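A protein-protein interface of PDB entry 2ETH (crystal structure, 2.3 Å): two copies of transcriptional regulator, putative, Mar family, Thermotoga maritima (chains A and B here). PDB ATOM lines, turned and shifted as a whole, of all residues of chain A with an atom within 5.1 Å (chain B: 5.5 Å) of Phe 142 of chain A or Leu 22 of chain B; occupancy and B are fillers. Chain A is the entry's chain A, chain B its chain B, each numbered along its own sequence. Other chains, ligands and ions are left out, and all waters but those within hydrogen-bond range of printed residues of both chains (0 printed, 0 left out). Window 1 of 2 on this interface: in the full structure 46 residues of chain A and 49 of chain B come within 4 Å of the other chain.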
ATOM      1  N   PHE A 119      -2.925  20.487  38.887  1.00  0.00           N
ATOM      2  CA  PHE A 119      -3.309  21.333  37.760  1.00  0.00           C
ATOM      3  C   PHE A 119      -2.961  22.812  38.033  1.00  0.00           C
ATOM      4  O   PHE A 119      -2.453  23.504  37.181  1.00  0.00           O
ATOM      5  CB  PHE A 119      -4.803  21.197  37.481  1.00  0.00           C
ATOM      6  CG  PHE A 119      -5.295  22.052  36.343  1.00  0.00           C
ATOM      7  CD1 PHE A 119      -5.145  21.636  35.022  1.00  0.00           C
ATOM      8  CD2 PHE A 119      -5.913  23.278  36.587  1.00  0.00           C
ATOM      9  CE1 PHE A 119      -5.598  22.428  33.956  1.00  0.00           C
ATOM     10  CE2 PHE A 119      -6.375  24.071  35.523  1.00  0.00           C
ATOM     11  CZ  PHE A 119      -6.214  23.636  34.207  1.00  0.00           C
ATOM     12  N   VAL A 138      -2.086  34.454  23.541  1.00  0.00           N
ATOM     13  CA  VAL A 138      -2.481  33.085  23.847  1.00  0.00           C
ATOM     14  C   VAL A 138      -3.963  33.011  24.285  1.00  0.00           C
ATOM     15  O   VAL A 138      -4.755  32.184  23.769  1.00  0.00           O
ATOM     16  CB  VAL A 138      -1.561  32.450  24.921  1.00  0.00           C
ATOM     17  CG1 VAL A 138      -2.121  31.135  25.387  1.00  0.00           C
ATOM     18  CG2 VAL A 138      -0.096  32.262  24.367  1.00  0.00           C
ATOM     19  N   SER A 139      -4.370  33.894  25.196  1.00  0.00           N
ATOM     20  CA  SER A 139      -5.704  33.830  25.726  1.00  0.00           C
ATOM     21  C   SER A 139      -6.755  34.355  24.763  1.00  0.00           C
ATOM     22  O   SER A 139      -7.911  33.904  24.790  1.00  0.00           O
ATOM     23  CB  SER A 139      -5.785  34.588  27.024  1.00  0.00           C
ATOM     24  OG  SER A 139      -5.919  35.932  26.752  1.00  0.00           O
ATOM     25  N   GLU A 140      -6.384  35.308  23.926  1.00  0.00           N
ATOM     26  CA  GLU A 140      -7.242  35.666  22.818  1.00  0.00           C
ATOM     27  C   GLU A 140      -7.559  34.479  21.921  1.00  0.00           C
ATOM     28  O   GLU A 140      -8.703  34.343  21.415  1.00  0.00           O
ATOM     29  CB  GLU A 140      -6.621  36.753  21.950  1.00  0.00           C
ATOM     30  CG  GLU A 140      -7.116  38.122  22.329  1.00  0.00           C
ATOM     31  CD  GLU A 140      -6.311  39.281  21.764  1.00  0.00           C
ATOM     32  OE1 GLU A 140      -5.389  39.100  20.921  1.00  0.00           O
ATOM     33  OE2 GLU A 140      -6.619  40.407  22.196  1.00  0.00           O
ATOM     34  N   GLY A 141      -6.531  33.696  21.635  1.00  0.00           N
ATOM     35  CA  GLY A 141      -6.679  32.506  20.836  1.00  0.00           C
ATOM     36  C   GLY A 141      -7.542  31.509  21.530  1.00  0.00           C
ATOM     37  O   GLY A 141      -8.415  30.928  20.930  1.00  0.00           O
ATOM     38  N   PHE A 142      -7.300  31.300  22.816  1.00  0.00           N
ATOM     39  CA  PHE A 142      -8.107  30.379  23.604  1.00  0.00           C
ATOM     40  C   PHE A 142      -9.590  30.747  23.606  1.00  0.00           C
ATOM     41  O   PHE A 142     -10.455  29.889  23.331  1.00  0.00           O
ATOM     42  CB  PHE A 142      -7.614  30.328  25.035  1.00  0.00           C
ATOM     43  CG  PHE A 142      -8.311  29.308  25.872  1.00  0.00           C
ATOM     44  CD1 PHE A 142      -8.052  27.961  25.678  1.00  0.00           C
ATOM     45  CD2 PHE A 142      -9.281  29.685  26.813  1.00  0.00           C
ATOM     46  CE1 PHE A 142      -8.716  27.002  26.426  1.00  0.00           C
ATOM     47  CE2 PHE A 142      -9.939  28.730  27.573  1.00  0.00           C
ATOM     48  CZ  PHE A 142      -9.634  27.378  27.386  1.00  0.00           C
ATOM     49  N   ASN A 143      -9.860  32.010  23.925  1.00  0.00           N
ATOM     50  CA  ASN A 143     -11.204  32.559  23.909  1.00  0.00           C
ATOM     51  C   ASN A 143     -11.909  32.417  22.550  1.00  0.00           C
ATOM     52  O   ASN A 143     -13.077  31.989  22.480  1.00  0.00           O
ATOM     53  CB  ASN A 143     -11.198  34.026  24.322  1.00  0.00           C
ATOM     54  CG  ASN A 143     -10.880  34.220  25.825  1.00  0.00           C
ATOM     55  OD1 ASN A 143     -10.806  33.284  26.556  1.00  0.00           O
ATOM     56  ND2 ASN A 143     -10.672  35.456  26.246  1.00  0.00           N
ATOM     57  N   ARG A 144     -11.199  32.770  21.492  1.00  0.00           N
ATOM     58  CA  ARG A 144     -11.730  32.650  20.167  1.00  0.00           C
ATOM     59  C   ARG A 144     -12.051  31.194  19.832  1.00  0.00           C
ATOM     60  O   ARG A 144     -13.015  30.938  19.187  1.00  0.00           O
ATOM     61  CB  ARG A 144     -10.774  33.207  19.150  1.00  0.00           C
ATOM     62  CG  ARG A 144     -11.303  33.205  17.749  1.00  0.00           C
ATOM     63  CD  ARG A 144     -12.426  34.185  17.516  1.00  0.00           C
ATOM     64  NE  ARG A 144     -11.923  35.514  17.218  1.00  0.00           N
ATOM     65  CZ  ARG A 144     -12.223  36.263  16.173  1.00  0.00           C
ATOM     66  NH1 ARG A 144     -13.034  35.869  15.226  1.00  0.00           N
ATOM     67  NH2 ARG A 144     -11.694  37.449  16.090  1.00  0.00           N
ATOM     68  N   MET A 145     -11.241  30.254  20.278  1.00  0.00           N
ATOM     69  CA  MET A 145     -11.517  28.826  20.005  1.00  0.00           C
ATOM     70  C   MET A 145     -12.740  28.337  20.773  1.00  0.00           C
ATOM     71  O   MET A 145     -13.578  27.593  20.245  1.00  0.00           O
ATOM     72  CB  MET A 145     -10.341  27.989  20.416  1.00  0.00           C
ATOM     73  CG  MET A 145     -10.504  26.563  20.080  1.00  0.00           C
ATOM     74  SD  MET A 145      -8.946  25.568  20.713  1.00  0.00           S
ATOM     75  CE  MET A 145      -9.136  26.098  22.579  1.00  0.00           C
ATOM     76  N   VAL A 146     -12.816  28.720  22.044  1.00  0.00           N
ATOM     77  CA  VAL A 146     -13.966  28.353  22.793  1.00  0.00           C
ATOM     78  C   VAL A 146     -15.218  28.978  22.199  1.00  0.00           C
ATOM     79  O   VAL A 146     -16.210  28.277  22.032  1.00  0.00           O
ATOM     80  CB  VAL A 146     -13.834  28.609  24.315  1.00  0.00           C
ATOM     81  CG1 VAL A 146     -15.174  28.281  24.973  1.00  0.00           C
ATOM     82  CG2 VAL A 146     -12.709  27.715  24.869  1.00  0.00           C
ATOM     83  N   GLU A 147     -15.207  30.265  21.861  1.00  0.00           N
ATOM     84  CA  GLU A 147     -16.383  30.839  21.256  1.00  0.00           C
ATOM     85  C   GLU A 147     -16.735  30.145  19.911  1.00  0.00           C
ATOM     86  O   GLU A 147     -17.882  29.779  19.696  1.00  0.00           O
ATOM     87  CB  GLU A 147     -16.227  32.333  21.043  1.00  0.00           C
ATOM     88  CG  GLU A 147     -15.757  33.129  22.243  1.00  0.00           C
ATOM     89  N   GLU B  17     -11.996  26.751  37.425  1.00  0.00           N
ATOM     90  CA  GLU B  17     -12.812  27.300  36.354  1.00  0.00           C
ATOM     91  C   GLU B  17     -12.175  27.008  34.989  1.00  0.00           C
ATOM     92  O   GLU B  17     -12.870  26.803  33.995  1.00  0.00           O
ATOM     93  CB  GLU B  17     -13.055  28.823  36.571  1.00  0.00           C
ATOM     94  N   ILE B  18     -10.856  26.966  34.942  1.00  0.00           N
ATOM     95  CA  ILE B  18     -10.135  26.727  33.676  1.00  0.00           C
ATOM     96  C   ILE B  18     -10.180  25.252  33.346  1.00  0.00           C
ATOM     97  O   ILE B  18     -10.337  24.846  32.182  1.00  0.00           O
ATOM     98  CB  ILE B  18      -8.657  27.176  33.793  1.00  0.00           C
ATOM     99  CG1 ILE B  18      -8.587  28.622  34.274  1.00  0.00           C
ATOM    100  CG2 ILE B  18      -7.913  26.953  32.488  1.00  0.00           C
ATOM    101  CD1 ILE B  18      -7.264  29.320  34.021  1.00  0.00           C
ATOM    102  N   PHE B  19     -10.040  24.461  34.396  1.00  0.00           N
ATOM    103  CA  PHE B  19     -10.225  23.022  34.341  1.00  0.00           C
ATOM    104  C   PHE B  19     -11.600  22.657  33.779  1.00  0.00           C
ATOM    105  O   PHE B  19     -11.697  21.897  32.823  1.00  0.00           O
ATOM    106  CB  PHE B  19     -10.068  22.452  35.742  1.00  0.00           C
ATOM    107  CG  PHE B  19      -9.618  21.003  35.798  1.00  0.00           C
ATOM    108  CD1 PHE B  19      -9.885  20.104  34.788  1.00  0.00           C
ATOM    109  CD2 PHE B  19      -8.945  20.534  36.920  1.00  0.00           C
ATOM    110  CE1 PHE B  19      -9.494  18.781  34.911  1.00  0.00           C
ATOM    111  CE2 PHE B  19      -8.531  19.224  37.016  1.00  0.00           C
ATOM    112  CZ  PHE B  19      -8.795  18.358  36.010  1.00  0.00           C
ATOM    113  N   LYS B  20     -12.655  23.202  34.381  1.00  0.00           N
ATOM    114  CA  LYS B  20     -14.014  22.973  33.906  1.00  0.00           C
ATOM    115  C   LYS B  20     -14.192  23.341  32.417  1.00  0.00           C
ATOM    116  O   LYS B  20     -14.885  22.635  31.697  1.00  0.00           O
ATOM    117  CB  LYS B  20     -15.031  23.772  34.762  1.00  0.00           C
ATOM    118  CG  LYS B  20     -15.358  23.188  36.079  1.00  0.00           C
ATOM    119  CD  LYS B  20     -16.517  23.893  36.686  1.00  0.00           C
ATOM    120  CE  LYS B  20     -16.660  23.696  38.210  1.00  0.00           C
ATOM    121  NZ  LYS B  20     -17.853  24.431  38.792  1.00  0.00           N
ATOM    122  N   THR B  21     -13.582  24.443  31.967  1.00  0.00           N
ATOM    123  CA  THR B  21     -13.710  24.908  30.575  1.00  0.00           C
ATOM    124  C   THR B  21     -12.922  23.968  29.646  1.00  0.00           C
ATOM    125  O   THR B  21     -13.402  23.553  28.610  1.00  0.00           O
ATOM    126  CB  THR B  21     -13.203  26.336  30.413  1.00  0.00           C
ATOM    127  OG1 THR B  21     -13.816  27.196  31.386  1.00  0.00           O
ATOM    128  CG2 THR B  21     -13.538  26.911  28.990  1.00  0.00           C
ATOM    129  N   LEU B  22     -11.714  23.604  30.046  1.00  0.00           N
ATOM    130  CA  LEU B  22     -10.891  22.662  29.274  1.00  0.00           C
ATOM    131  C   LEU B  22     -11.607  21.342  29.066  1.00  0.00           C
ATOM    132  O   LEU B  22     -11.618  20.799  27.969  1.00  0.00           O
ATOM    133  CB  LEU B  22      -9.556  22.434  29.980  1.00  0.00           C
ATOM    134  CG  LEU B  22      -8.550  23.574  29.757  1.00  0.00           C
ATOM    135  CD1 LEU B  22      -7.361  23.448  30.718  1.00  0.00           C
ATOM    136  CD2 LEU B  22      -8.065  23.621  28.305  1.00  0.00           C
ATOM    137  N   PHE B  23     -12.235  20.852  30.125  1.00  0.00           N
ATOM    138  CA  PHE B  23     -12.959  19.588  30.120  1.00  0.00           C
ATOM    139  C   PHE B  23     -14.239  19.610  29.295  1.00  0.00           C
ATOM    140  O   PHE B  23     -14.571  18.632  28.673  1.00  0.00           O
ATOM    141  CB  PHE B  23     -13.298  19.177  31.568  1.00  0.00           C
ATOM    142  CG  PHE B  23     -13.770  17.763  31.683  1.00  0.00           C
ATOM    143  CD1 PHE B  23     -12.874  16.739  31.717  1.00  0.00           C
ATOM    144  CD2 PHE B  23     -15.123  17.460  31.728  1.00  0.00           C
ATOM    145  CE1 PHE B  23     -13.304  15.440  31.788  1.00  0.00           C
ATOM    146  CE2 PHE B  23     -15.538  16.165  31.793  1.00  0.00           C
ATOM    147  CZ  PHE B  23     -14.640  15.164  31.832  1.00  0.00           C
ATOM    148  N   SER B  24     -14.994  20.694  29.352  1.00  0.00           N
ATOM    149  CA  SER B  24     -16.114  20.920  28.436  1.00  0.00           C
ATOM    150  C   SER B  24     -15.683  20.919  26.970  1.00  0.00           C
ATOM    151  O   SER B  24     -16.350  20.370  26.109  1.00  0.00           O
ATOM    152  CB  SER B  24     -16.745  22.271  28.741  1.00  0.00           C
ATOM    153  OG  SER B  24     -17.116  22.291  30.103  1.00  0.00           O
ATOM    154  N   LEU B  25     -14.566  21.578  26.695  1.00  0.00           N
ATOM    155  CA  LEU B  25     -13.986  21.572  25.372  1.00  0.00           C
ATOM    156  C   LEU B  25     -13.689  20.114  24.974  1.00  0.00           C
ATOM    157  O   LEU B  25     -14.266  19.606  24.015  1.00  0.00           O
ATOM    158  CB  LEU B  25     -12.727  22.445  25.381  1.00  0.00           C
ATOM    159  CG  LEU B  25     -12.208  22.993  24.080  1.00  0.00           C
ATOM    160  CD1 LEU B  25     -13.296  23.804  23.368  1.00  0.00           C
ATOM    161  CD2 LEU B  25     -10.957  23.830  24.387  1.00  0.00           C
ATOM    162  N   VAL B  26     -12.850  19.426  25.747  1.00  0.00           N
ATOM    163  CA  VAL B  26     -12.568  17.995  25.515  1.00  0.00           C
ATOM    164  C   VAL B  26     -13.864  17.205  25.274  1.00  0.00           C
ATOM    165  O   VAL B  26     -13.921  16.391  24.340  1.00  0.00           O
ATOM    166  CB  VAL B  26     -11.813  17.359  26.690  1.00  0.00           C
ATOM    167  CG1 VAL B  26     -11.828  15.818  26.567  1.00  0.00           C
ATOM    168  CG2 VAL B  26     -10.372  17.918  26.787  1.00  0.00           C
ATOM    169  N   MET B  27     -14.885  17.464  26.104  1.00  0.00           N
ATOM    170  CA  MET B  27     -16.222  16.891  25.938  1.00  0.00           C
ATOM    171  C   MET B  27     -16.733  17.099  24.547  1.00  0.00           C
ATOM    172  O   MET B  27     -17.320  16.180  23.999  1.00  0.00           O
ATOM    173  CB  MET B  27     -17.247  17.491  26.927  1.00  0.00           C
ATOM    174  CG  MET B  27     -17.333  16.787  28.302  1.00  0.00           C
ATOM    175  SD  MET B  27     -18.483  17.666  29.682  1.00  0.00           S
ATOM    176  CE  MET B  27     -20.232  16.998  29.171  1.00  0.00           C
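Phe 119 of chain A touches Phe 19 of chain B.
CD1 of Leu 22 of chain B touches CZ of Phe 119 of chain A, at 3.7 Å.
Leu 22 of chain B touches Phe 142 of chain A (CD2 to CE1, 3.9 Å).
Met 145 of chain A touches Leu 25 of chain B (CE to CD2, 3.4 Å).
Of chain B, only Leu 22 (3.9 Å) comes within 4 Å of Phe 142 of chain A.
Of chain A, only Phe 119 and Phe 142 come within 4 Å of Leu 22 of chain B.
Of the printed residues of chain A, Phe 19 of chain B touches Phe 119.
Printed residues of chain B within 4 Å of Met 145 of chain A: Leu 25 (3.4 Å).
Of the printed residues of chain B, Phe 119 of chain A touches Phe 19 (3.9 Å) and Leu 22 (3.7 Å).
Arg 144 of chain A touches none of the printed residues of chain B.
The nearest residue of chain B that does not touch Phe 142 of chain A is Thr 21 of chain B (4.2 Å).
The nearest printed residue of chain B that does not touch Phe 119 of chain A is Ile 18 of chain B (4.1 Å).
No position is printed for both chains.
Of the 11 printed residues of chain A, 3 touch a printed residue of chain B.
Hydrophobic or aromatic side chains of chain A that line the printed part of chain B: Phe 119, Phe 142 and Met 145.
Of the 11 printed residues of chain B, 3 touch a printed residue of chain A.
Printed residues of chain B that touch a printed residue of chain A: Phe 19, Leu 22 and Leu 25.
Among the printed residues, 4 pairs touch across the chains.
Among the printed residues, no Asp or Glu carboxylate lies within 4 Å of a Lys or Arg side-chain nitrogen of the other chain.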
